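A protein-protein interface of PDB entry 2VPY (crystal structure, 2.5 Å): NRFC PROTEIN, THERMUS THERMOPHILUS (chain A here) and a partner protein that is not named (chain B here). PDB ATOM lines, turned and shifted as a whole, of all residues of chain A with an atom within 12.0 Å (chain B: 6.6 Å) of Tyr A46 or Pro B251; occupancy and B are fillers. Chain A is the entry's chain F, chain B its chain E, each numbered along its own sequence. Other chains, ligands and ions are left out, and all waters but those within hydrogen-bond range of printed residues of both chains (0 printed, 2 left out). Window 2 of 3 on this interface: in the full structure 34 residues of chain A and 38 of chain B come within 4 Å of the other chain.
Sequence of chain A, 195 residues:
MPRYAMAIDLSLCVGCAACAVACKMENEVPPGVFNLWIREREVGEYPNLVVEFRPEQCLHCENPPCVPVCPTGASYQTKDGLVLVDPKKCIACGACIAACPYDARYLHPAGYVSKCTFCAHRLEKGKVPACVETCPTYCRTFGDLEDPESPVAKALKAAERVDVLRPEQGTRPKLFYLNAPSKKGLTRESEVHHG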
ATOM      1  N   GLU A  42       0.109 -12.066   1.165  1.00  0.00           N
ATOM      2  CA  GLU A  42      -0.816 -12.128   2.311  1.00  0.00           C
ATOM      3  C   GLU A  42      -1.201 -13.608   2.530  1.00  0.00           C
ATOM      4  O   GLU A  42      -1.246 -14.384   1.582  1.00  0.00           O
ATOM      5  CB  GLU A  42      -2.075 -11.246   2.093  1.00  0.00           C
ATOM      6  CG  GLU A  42      -3.086 -11.742   1.064  1.00  0.00           C
ATOM      7  CD  GLU A  42      -4.205 -10.730   0.792  1.00  0.00           C
ATOM      8  OE1 GLU A  42      -5.375 -11.032   1.144  1.00  0.00           O
ATOM      9  OE2 GLU A  42      -3.919  -9.645   0.227  1.00  0.00           O
ATOM     10  N   VAL A  43      -1.410 -13.995   3.787  1.00  0.00           N
ATOM     11  CA  VAL A  43      -1.786 -15.363   4.202  1.00  0.00           C
ATOM     12  C   VAL A  43      -2.988 -14.936   4.975  1.00  0.00           C
ATOM     13  O   VAL A  43      -2.896 -14.208   5.967  1.00  0.00           O
ATOM     14  CB  VAL A  43      -0.715 -15.991   5.044  1.00  0.00           C
ATOM     15  CG1 VAL A  43      -1.060 -17.424   5.298  1.00  0.00           C
ATOM     16  CG2 VAL A  43       0.585 -15.931   4.304  1.00  0.00           C
ATOM     17  N   GLY A  44      -4.115 -15.466   4.553  1.00  0.00           N
ATOM     18  CA  GLY A  44      -5.308 -14.813   5.007  1.00  0.00           C
ATOM     19  C   GLY A  44      -6.426 -15.114   5.918  1.00  0.00           C
ATOM     20  O   GLY A  44      -6.373 -16.086   6.628  1.00  0.00           O
ATOM     21  N   GLU A  45      -7.418 -14.220   5.890  1.00  0.00           N
ATOM     22  CA  GLU A  45      -8.643 -14.269   6.700  1.00  0.00           C
ATOM     23  C   GLU A  45      -8.541 -13.487   8.023  1.00  0.00           C
ATOM     24  O   GLU A  45      -7.813 -13.882   8.935  1.00  0.00           O
ATOM     25  CB  GLU A  45      -9.038 -15.712   6.960  1.00  0.00           C
ATOM     26  CG  GLU A  45      -9.457 -16.487   5.718  1.00  0.00           C
ATOM     27  CD  GLU A  45     -10.925 -16.288   5.365  1.00  0.00           C
ATOM     28  OE1 GLU A  45     -11.296 -15.162   4.952  1.00  0.00           O
ATOM     29  OE2 GLU A  45     -11.703 -17.263   5.516  1.00  0.00           O
ATOM     30  N   TYR A  46      -9.326 -12.411   8.109  1.00  0.00           N
ATOM     31  CA  TYR A  46      -9.383 -11.430   9.222  1.00  0.00           C
ATOM     32  C   TYR A  46      -8.683 -11.538  10.585  1.00  0.00           C
ATOM     33  O   TYR A  46      -7.643 -10.879  10.776  1.00  0.00           O
ATOM     34  CB  TYR A  46     -10.838 -10.968   9.490  1.00  0.00           C
ATOM     35  CG  TYR A  46     -11.029 -10.156  10.777  1.00  0.00           C
ATOM     36  CD1 TYR A  46     -10.131  -9.149  11.128  1.00  0.00           C
ATOM     37  CD2 TYR A  46     -12.106 -10.405  11.639  1.00  0.00           C
ATOM     38  CE1 TYR A  46     -10.287  -8.409  12.305  1.00  0.00           C
ATOM     39  CE2 TYR A  46     -12.278  -9.663  12.828  1.00  0.00           C
ATOM     40  CZ  TYR A  46     -11.364  -8.667  13.155  1.00  0.00           C
ATOM     41  OH  TYR A  46     -11.519  -7.948  14.324  1.00  0.00           O
ATOM     42  N   PRO A  47      -9.243 -12.313  11.560  1.00  0.00           N
ATOM     43  CA  PRO A  47      -8.604 -12.422  12.877  1.00  0.00           C
ATOM     44  C   PRO A  47      -7.198 -12.957  12.795  1.00  0.00           C
ATOM     45  O   PRO A  47      -6.402 -12.820  13.737  1.00  0.00           O
ATOM     46  CB  PRO A  47      -9.531 -13.361  13.663  1.00  0.00           C
ATOM     47  CG  PRO A  47     -10.210 -14.177  12.623  1.00  0.00           C
ATOM     48  CD  PRO A  47     -10.348 -13.278  11.433  1.00  0.00           C
ATOM     49  N   ASN A  48      -6.904 -13.501  11.624  1.00  0.00           N
ATOM     50  CA  ASN A  48      -5.648 -14.158  11.354  1.00  0.00           C
ATOM     51  C   ASN A  48      -4.974 -13.798  10.021  1.00  0.00           C
ATOM     52  O   ASN A  48      -4.567 -14.681   9.276  1.00  0.00           O
ATOM     53  CB  ASN A  48      -5.903 -15.677  11.425  1.00  0.00           C
ATOM     54  CG  ASN A  48      -6.519 -16.135  12.779  1.00  0.00           C
ATOM     55  OD1 ASN A  48      -5.907 -15.974  13.842  1.00  0.00           O
ATOM     56  ND2 ASN A  48      -7.720 -16.716  12.728  1.00  0.00           N
ATOM     57  N   LEU A  49      -4.867 -12.508   9.735  1.00  0.00           N
ATOM     58  CA  LEU A  49      -4.228 -12.011   8.525  1.00  0.00           C
ATOM     59  C   LEU A  49      -2.727 -11.889   8.823  1.00  0.00           C
ATOM     60  O   LEU A  49      -2.365 -11.428   9.902  1.00  0.00           O
ATOM     61  CB  LEU A  49      -4.771 -10.612   8.203  1.00  0.00           C
ATOM     62  CG  LEU A  49      -5.213 -10.160   6.827  1.00  0.00           C
ATOM     63  CD1 LEU A  49      -5.448 -11.368   5.971  1.00  0.00           C
ATOM     64  CD2 LEU A  49      -6.465  -9.312   6.955  1.00  0.00           C
ATOM     65  N   VAL A  50      -1.879 -12.306   7.882  1.00  0.00           N
ATOM     66  CA  VAL A  50      -0.417 -12.179   7.980  1.00  0.00           C
ATOM     67  C   VAL A  50       0.153 -11.696   6.612  1.00  0.00           C
ATOM     68  O   VAL A  50      -0.289 -12.179   5.571  1.00  0.00           O
ATOM     69  CB  VAL A  50       0.247 -13.540   8.431  1.00  0.00           C
ATOM     70  CG1 VAL A  50       1.782 -13.533   8.202  1.00  0.00           C
ATOM     71  CG2 VAL A  50      -0.053 -13.767   9.915  1.00  0.00           C
ATOM     72  N   VAL A  51       1.051 -10.700   6.606  1.00  0.00           N
ATOM     73  CA  VAL A  51       1.692 -10.225   5.361  1.00  0.00           C
ATOM     74  C   VAL A  51       3.206 -10.397   5.529  1.00  0.00           C
ATOM     75  O   VAL A  51       3.807  -9.972   6.526  1.00  0.00           O
ATOM     76  CB  VAL A  51       1.413  -8.691   4.960  1.00  0.00           C
ATOM     77  CG1 VAL A  51       1.967  -8.400   3.528  1.00  0.00           C
ATOM     78  CG2 VAL A  51      -0.065  -8.378   4.982  1.00  0.00           C
ATOM     79  N   VAL B 234      -3.161  -0.789  15.429  1.00  0.00           N
ATOM     80  CA  VAL B 234      -3.476  -0.017  14.243  1.00  0.00           C
ATOM     81  C   VAL B 234      -5.007   0.034  14.106  1.00  0.00           C
ATOM     82  O   VAL B 234      -5.670  -1.000  14.218  1.00  0.00           O
ATOM     83  CB  VAL B 234      -2.751  -0.668  13.012  1.00  0.00           C
ATOM     84  CG1 VAL B 234      -3.137  -0.009  11.687  1.00  0.00           C
ATOM     85  CG2 VAL B 234      -1.248  -0.539  13.231  1.00  0.00           C
ATOM     86  N   VAL B 235      -5.563   1.239  13.961  1.00  0.00           N
ATOM     87  CA  VAL B 235      -7.023   1.453  13.792  1.00  0.00           C
ATOM     88  C   VAL B 235      -7.121   1.933  12.339  1.00  0.00           C
ATOM     89  O   VAL B 235      -6.573   2.987  11.977  1.00  0.00           O
ATOM     90  CB  VAL B 235      -7.583   2.518  14.788  1.00  0.00           C
ATOM     91  CG1 VAL B 235      -9.084   2.631  14.625  1.00  0.00           C
ATOM     92  CG2 VAL B 235      -7.256   2.122  16.246  1.00  0.00           C
ATOM     93  N   ASP B 236      -7.844   1.174  11.515  1.00  0.00           N
ATOM     94  CA  ASP B 236      -7.846   1.450  10.076  1.00  0.00           C
ATOM     95  C   ASP B 236      -8.738   0.383   9.404  1.00  0.00           C
ATOM     96  O   ASP B 236      -8.652  -0.795   9.748  1.00  0.00           O
ATOM     97  CB  ASP B 236      -6.370   1.270   9.622  1.00  0.00           C
ATOM     98  CG  ASP B 236      -6.053   1.759   8.185  1.00  0.00           C
ATOM     99  OD1 ASP B 236      -6.923   1.743   7.306  1.00  0.00           O
ATOM    100  OD2 ASP B 236      -4.882   2.137   7.923  1.00  0.00           O
ATOM    101  N   PRO B 237      -9.608   0.779   8.449  1.00  0.00           N
ATOM    102  CA  PRO B 237     -10.468  -0.209   7.774  1.00  0.00           C
ATOM    103  C   PRO B 237      -9.708  -1.125   6.789  1.00  0.00           C
ATOM    104  O   PRO B 237     -10.271  -2.066   6.229  1.00  0.00           O
ATOM    105  CB  PRO B 237     -11.504   0.661   7.045  1.00  0.00           C
ATOM    106  CG  PRO B 237     -10.778   1.983   6.834  1.00  0.00           C
ATOM    107  CD  PRO B 237     -10.033   2.151   8.134  1.00  0.00           C
ATOM    108  N   ARG B 238      -8.433  -0.835   6.579  1.00  0.00           N
ATOM    109  CA  ARG B 238      -7.600  -1.594   5.646  1.00  0.00           C
ATOM    110  C   ARG B 238      -6.467  -2.315   6.393  1.00  0.00           C
ATOM    111  O   ARG B 238      -5.883  -1.730   7.307  1.00  0.00           O
ATOM    112  CB  ARG B 238      -7.001  -0.615   4.610  1.00  0.00           C
ATOM    113  CG  ARG B 238      -6.176  -1.256   3.514  1.00  0.00           C
ATOM    114  CD  ARG B 238      -5.538  -0.215   2.587  1.00  0.00           C
ATOM    115  NE  ARG B 238      -4.585   0.659   3.258  1.00  0.00           N
ATOM    116  CZ  ARG B 238      -3.264   0.527   3.195  1.00  0.00           C
ATOM    117  NH1 ARG B 238      -2.732  -0.466   2.485  1.00  0.00           N
ATOM    118  NH2 ARG B 238      -2.472   1.407   3.795  1.00  0.00           N
ATOM    119  N   PHE B 239      -6.155  -3.565   6.077  1.00  0.00           N
ATOM    120  CA  PHE B 239      -4.998  -4.213   6.747  1.00  0.00           C
ATOM    121  C   PHE B 239      -3.814  -3.692   6.020  1.00  0.00           C
ATOM    122  O   PHE B 239      -3.394  -4.171   5.065  1.00  0.00           O
ATOM    123  CB  PHE B 239      -4.842  -5.730   6.512  1.00  0.00           C
ATOM    124  CG  PHE B 239      -3.991  -6.435   7.576  1.00  0.00           C
ATOM    125  CD1 PHE B 239      -4.421  -6.413   8.919  1.00  0.00           C
ATOM    126  CD2 PHE B 239      -2.800  -7.100   7.266  1.00  0.00           C
ATOM    127  CE1 PHE B 239      -3.664  -7.052   9.940  1.00  0.00           C
ATOM    128  CE2 PHE B 239      -2.043  -7.751   8.287  1.00  0.00           C
ATOM    129  CZ  PHE B 239      -2.472  -7.723   9.610  1.00  0.00           C
ATOM    130  N   TRP B 249      -5.241  -5.176  15.435  1.00  0.00           N
ATOM    131  CA  TRP B 249      -5.709  -4.415  14.278  1.00  0.00           C
ATOM    132  C   TRP B 249      -7.191  -4.162  14.532  1.00  0.00           C
ATOM    133  O   TRP B 249      -7.932  -5.110  14.712  1.00  0.00           O
ATOM    134  CB  TRP B 249      -5.574  -5.192  12.962  1.00  0.00           C
ATOM    135  CG  TRP B 249      -6.255  -4.499  11.785  1.00  0.00           C
ATOM    136  CD1 TRP B 249      -6.245  -3.164  11.496  1.00  0.00           C
ATOM    137  CD2 TRP B 249      -7.030  -5.122  10.740  1.00  0.00           C
ATOM    138  NE1 TRP B 249      -6.961  -2.915  10.351  1.00  0.00           N
ATOM    139  CE2 TRP B 249      -7.457  -4.093   9.866  1.00  0.00           C
ATOM    140  CE3 TRP B 249      -7.409  -6.451  10.464  1.00  0.00           C
ATOM    141  CZ2 TRP B 249      -8.237  -4.347   8.720  1.00  0.00           C
ATOM    142  CZ3 TRP B 249      -8.190  -6.707   9.318  1.00  0.00           C
ATOM    143  CH2 TRP B 249      -8.594  -5.650   8.466  1.00  0.00           C
ATOM    144  N   LEU B 250      -7.643  -2.911  14.603  1.00  0.00           N
ATOM    145  CA  LEU B 250      -9.088  -2.703  14.797  1.00  0.00           C
ATOM    146  C   LEU B 250      -9.646  -2.292  13.421  1.00  0.00           C
ATOM    147  O   LEU B 250      -9.424  -1.177  12.961  1.00  0.00           O
ATOM    148  CB  LEU B 250      -9.390  -1.622  15.853  1.00  0.00           C
ATOM    149  CG  LEU B 250      -8.600  -1.481  17.173  1.00  0.00           C
ATOM    150  CD1 LEU B 250      -9.572  -0.953  18.214  1.00  0.00           C
ATOM    151  CD2 LEU B 250      -7.983  -2.798  17.674  1.00  0.00           C
ATOM    152  N   PRO B 251     -10.371  -3.196  12.739  1.00  0.00           N
ATOM    153  CA  PRO B 251     -10.862  -2.736  11.431  1.00  0.00           C
ATOM    154  C   PRO B 251     -12.096  -1.846  11.500  1.00  0.00           C
ATOM    155  O   PRO B 251     -13.195  -2.254  11.140  1.00  0.00           O
ATOM    156  CB  PRO B 251     -11.104  -4.032  10.671  1.00  0.00           C
ATOM    157  CG  PRO B 251     -11.530  -4.991  11.763  1.00  0.00           C
ATOM    158  CD  PRO B 251     -10.794  -4.579  13.025  1.00  0.00           C
ATOM    159  N   ILE B 252     -11.871  -0.613  11.926  1.00  0.00           N
ATOM    160  CA  ILE B 252     -12.926   0.352  12.141  1.00  0.00           C
ATOM    161  C   ILE B 252     -13.763   0.713  10.917  1.00  0.00           C
ATOM    162  O   ILE B 252     -13.289   0.669   9.780  1.00  0.00           O
ATOM    163  CB  ILE B 252     -12.307   1.628  12.797  1.00  0.00           C
ATOM    164  CG1 ILE B 252     -13.382   2.403  13.566  1.00  0.00           C
ATOM    165  CG2 ILE B 252     -11.576   2.447  11.735  1.00  0.00           C
ATOM    166  CD1 ILE B 252     -12.830   3.563  14.412  1.00  0.00           C
ATOM    167  N   LYS B 253     -15.026   1.032  11.157  1.00  0.00           N
ATOM    168  CA  LYS B 253     -15.893   1.450  10.080  1.00  0.00           C
ATOM    169  C   LYS B 253     -15.469   2.868   9.721  1.00  0.00           C
ATOM    170  O   LYS B 253     -15.330   3.736  10.598  1.00  0.00           O
ATOM    171  CB  LYS B 253     -17.337   1.423  10.511  1.00  0.00           C
ATOM    172  CG  LYS B 253     -18.255   1.711   9.391  1.00  0.00           C
ATOM    173  CD  LYS B 253     -19.629   1.681   9.913  1.00  0.00           C
ATOM    174  CE  LYS B 253     -20.481   2.672   9.185  1.00  0.00           C
ATOM    175  NZ  LYS B 253     -21.853   2.496   9.684  1.00  0.00           N
ATOM    176  N   PRO B 254     -15.257   3.131   8.425  1.00  0.00           N
ATOM    177  CA  PRO B 254     -14.827   4.487   8.063  1.00  0.00           C
ATOM    178  C   PRO B 254     -15.675   5.676   8.550  1.00  0.00           C
ATOM    179  O   PRO B 254     -16.913   5.616   8.531  1.00  0.00           O
ATOM    180  CB  PRO B 254     -14.686   4.455   6.540  1.00  0.00           C
ATOM    181  CG  PRO B 254     -15.037   3.051   6.105  1.00  0.00           C
ATOM    182  CD  PRO B 254     -15.321   2.200   7.291  1.00  0.00           C
ATOM    183  N   THR B 305     -19.043   2.127  15.457  1.00  0.00           N
ATOM    184  CA  THR B 305     -17.687   1.752  15.166  1.00  0.00           C
ATOM    185  C   THR B 305     -17.477   0.342  14.619  1.00  0.00           C
ATOM    186  O   THR B 305     -16.655   0.088  13.726  1.00  0.00           O
ATOM    187  CB  THR B 305     -16.960   2.020  16.533  1.00  0.00           C
ATOM    188  OG1 THR B 305     -16.046   3.108  16.424  1.00  0.00           O
ATOM    189  CG2 THR B 305     -16.328   0.812  17.067  1.00  0.00           C
ATOM    190  N   GLU B 306     -18.289  -0.544  15.163  1.00  0.00           N
ATOM    191  CA  GLU B 306     -18.287  -1.963  14.893  1.00  0.00           C
ATOM    192  C   GLU B 306     -17.085  -2.625  15.587  1.00  0.00           C
ATOM    193  O   GLU B 306     -16.799  -3.790  15.336  1.00  0.00           O
ATOM    194  CB  GLU B 306     -18.317  -2.268  13.400  1.00  0.00           C
ATOM    195  CG  GLU B 306     -19.417  -1.537  12.650  1.00  0.00           C
ATOM    196  CD  GLU B 306     -19.616  -2.075  11.252  1.00  0.00           C
ATOM    197  OE1 GLU B 306     -18.728  -2.820  10.791  1.00  0.00           O
ATOM    198  OE2 GLU B 306     -20.652  -1.749  10.628  1.00  0.00           O
ATOM    199  N   ILE B 307     -16.368  -1.884  16.438  1.00  0.00           N
ATOM    200  CA  ILE B 307     -15.264  -2.463  17.208  1.00  0.00           C
ATOM    201  C   ILE B 307     -15.982  -2.954  18.492  1.00  0.00           C
ATOM    202  O   ILE B 307     -16.714  -2.192  19.136  1.00  0.00           O
ATOM    203  CB  ILE B 307     -14.123  -1.411  17.490  1.00  0.00           C
ATOM    204  CG1 ILE B 307     -13.614  -0.887  16.151  1.00  0.00           C
ATOM    205  CG2 ILE B 307     -12.969  -2.042  18.317  1.00  0.00           C
ATOM    206  CD1 ILE B 307     -13.096  -1.980  15.203  1.00  0.00           C
ATOM    207  N   PRO B 308     -15.809  -4.247  18.855  1.00  0.00           N
ATOM    208  CA  PRO B 308     -16.488  -4.745  20.060  1.00  0.00           C
ATOM    209  C   PRO B 308     -16.117  -4.007  21.353  1.00  0.00           C
ATOM    210  O   PRO B 308     -14.950  -3.704  21.599  1.00  0.00           O
ATOM    211  CB  PRO B 308     -16.161  -6.255  20.073  1.00  0.00           C
ATOM    212  CG  PRO B 308     -15.557  -6.540  18.696  1.00  0.00           C
ATOM    213  CD  PRO B 308     -14.866  -5.248  18.328  1.00  0.00           C
ATOM    214  N   ALA B 686      -7.863  -9.697   0.181  1.00  0.00           N
ATOM    215  CA  ALA B 686      -8.516  -9.587   1.561  1.00  0.00           C
ATOM    216  C   ALA B 686      -8.199  -8.675   2.816  1.00  0.00           C
ATOM    217  O   ALA B 686      -8.684  -8.908   3.960  1.00  0.00           O
ATOM    218  CB  ALA B 686      -8.481 -10.993   2.058  1.00  0.00           C
ATOM    219  N   ARG B 689     -12.161  -3.836   4.370  1.00  0.00           N
ATOM    220  CA  ARG B 689     -13.576  -4.084   4.612  1.00  0.00           C
ATOM    221  C   ARG B 689     -14.312  -4.095   3.251  1.00  0.00           C
ATOM    222  O   ARG B 689     -13.760  -3.684   2.227  1.00  0.00           O
ATOM    223  CB  ARG B 689     -14.178  -3.032   5.539  1.00  0.00           C
ATOM    224  CG  ARG B 689     -13.686  -3.122   6.972  1.00  0.00           C
ATOM    225  CD  ARG B 689     -13.893  -1.800   7.645  1.00  0.00           C
ATOM    226  NE  ARG B 689     -15.296  -1.425   7.528  1.00  0.00           N
ATOM    227  CZ  ARG B 689     -16.236  -1.761   8.408  1.00  0.00           C
ATOM    228  NH1 ARG B 689     -15.916  -2.470   9.483  1.00  0.00           N
ATOM    229  NH2 ARG B 689     -17.506  -1.429   8.209  1.00  0.00           N
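Hydrophobic or aromatic side chains of chain B within 4 Å of the printed part of chain A: Phe B239, Trp B249, Pro B251 and Ala B686.
Among the printed residues, 7 pairs touch across the chains.
Tyr A46 touches two residues of chain B.
Pro B251 touches just one residue of chain A: Tyr A46 (3.7 Å).
No residue of chain A comes within 4 Å of Val B235.
Pro B237 touches none of the printed residues of chain A.
Trp B249 touches just these residues of chain A: Tyr A46 (3.6 Å) and Leu A49 (3.9 Å).
No residue of chain A comes within 4 Å of Leu B250.
No residue of chain A comes within 4 Å of Ile B252.
No residue of chain A comes within 4 Å of Glu B306.
Of the printed residues of chain A, Phe B239 touches Leu A49 and Val A51.
Of the printed residues of chain A, Ala B686 touches Glu A42 (3.0 Å) and Leu A49 (3.7 Å).
Of the printed residues of chain B, Leu A49 touches Phe B239, Trp B249 and Ala B686.
The nearest residue of chain A that does not touch Pro B251 is Pro A47 (7.7 Å).
The nearest printed residue of chain B that does not touch Leu A49 is Arg B238 (7.0 Å).
The indole nitrogen (NE1) of Trp B249 sits at hydrogen-bond distance from the backbone carbonyl oxygen (O) of Asp B236, at 2.8 Å.
The backbone carbonyl oxygen of Arg B238 sits at hydrogen-bond distance from the indole nitrogen of Trp B249.
The guanidinium group of Arg B689 sits at hydrogen-bond distance from the backbone carbonyl oxygen of Pro B251, at 3.2 Å.
Among the printed residues, merely in contact across the chains: Tyr A46 with Trp B249, Tyr A46 with Pro B251, Leu A49 with Phe B239, Leu A49 with Ala B686, Val A51 with Phe B239 and Leu A49 with Trp B249.
The backbone NH of Ala B686 sits at hydrogen-bond distance from the side-chain carboxylate of Glu A42 (3.0 Å).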
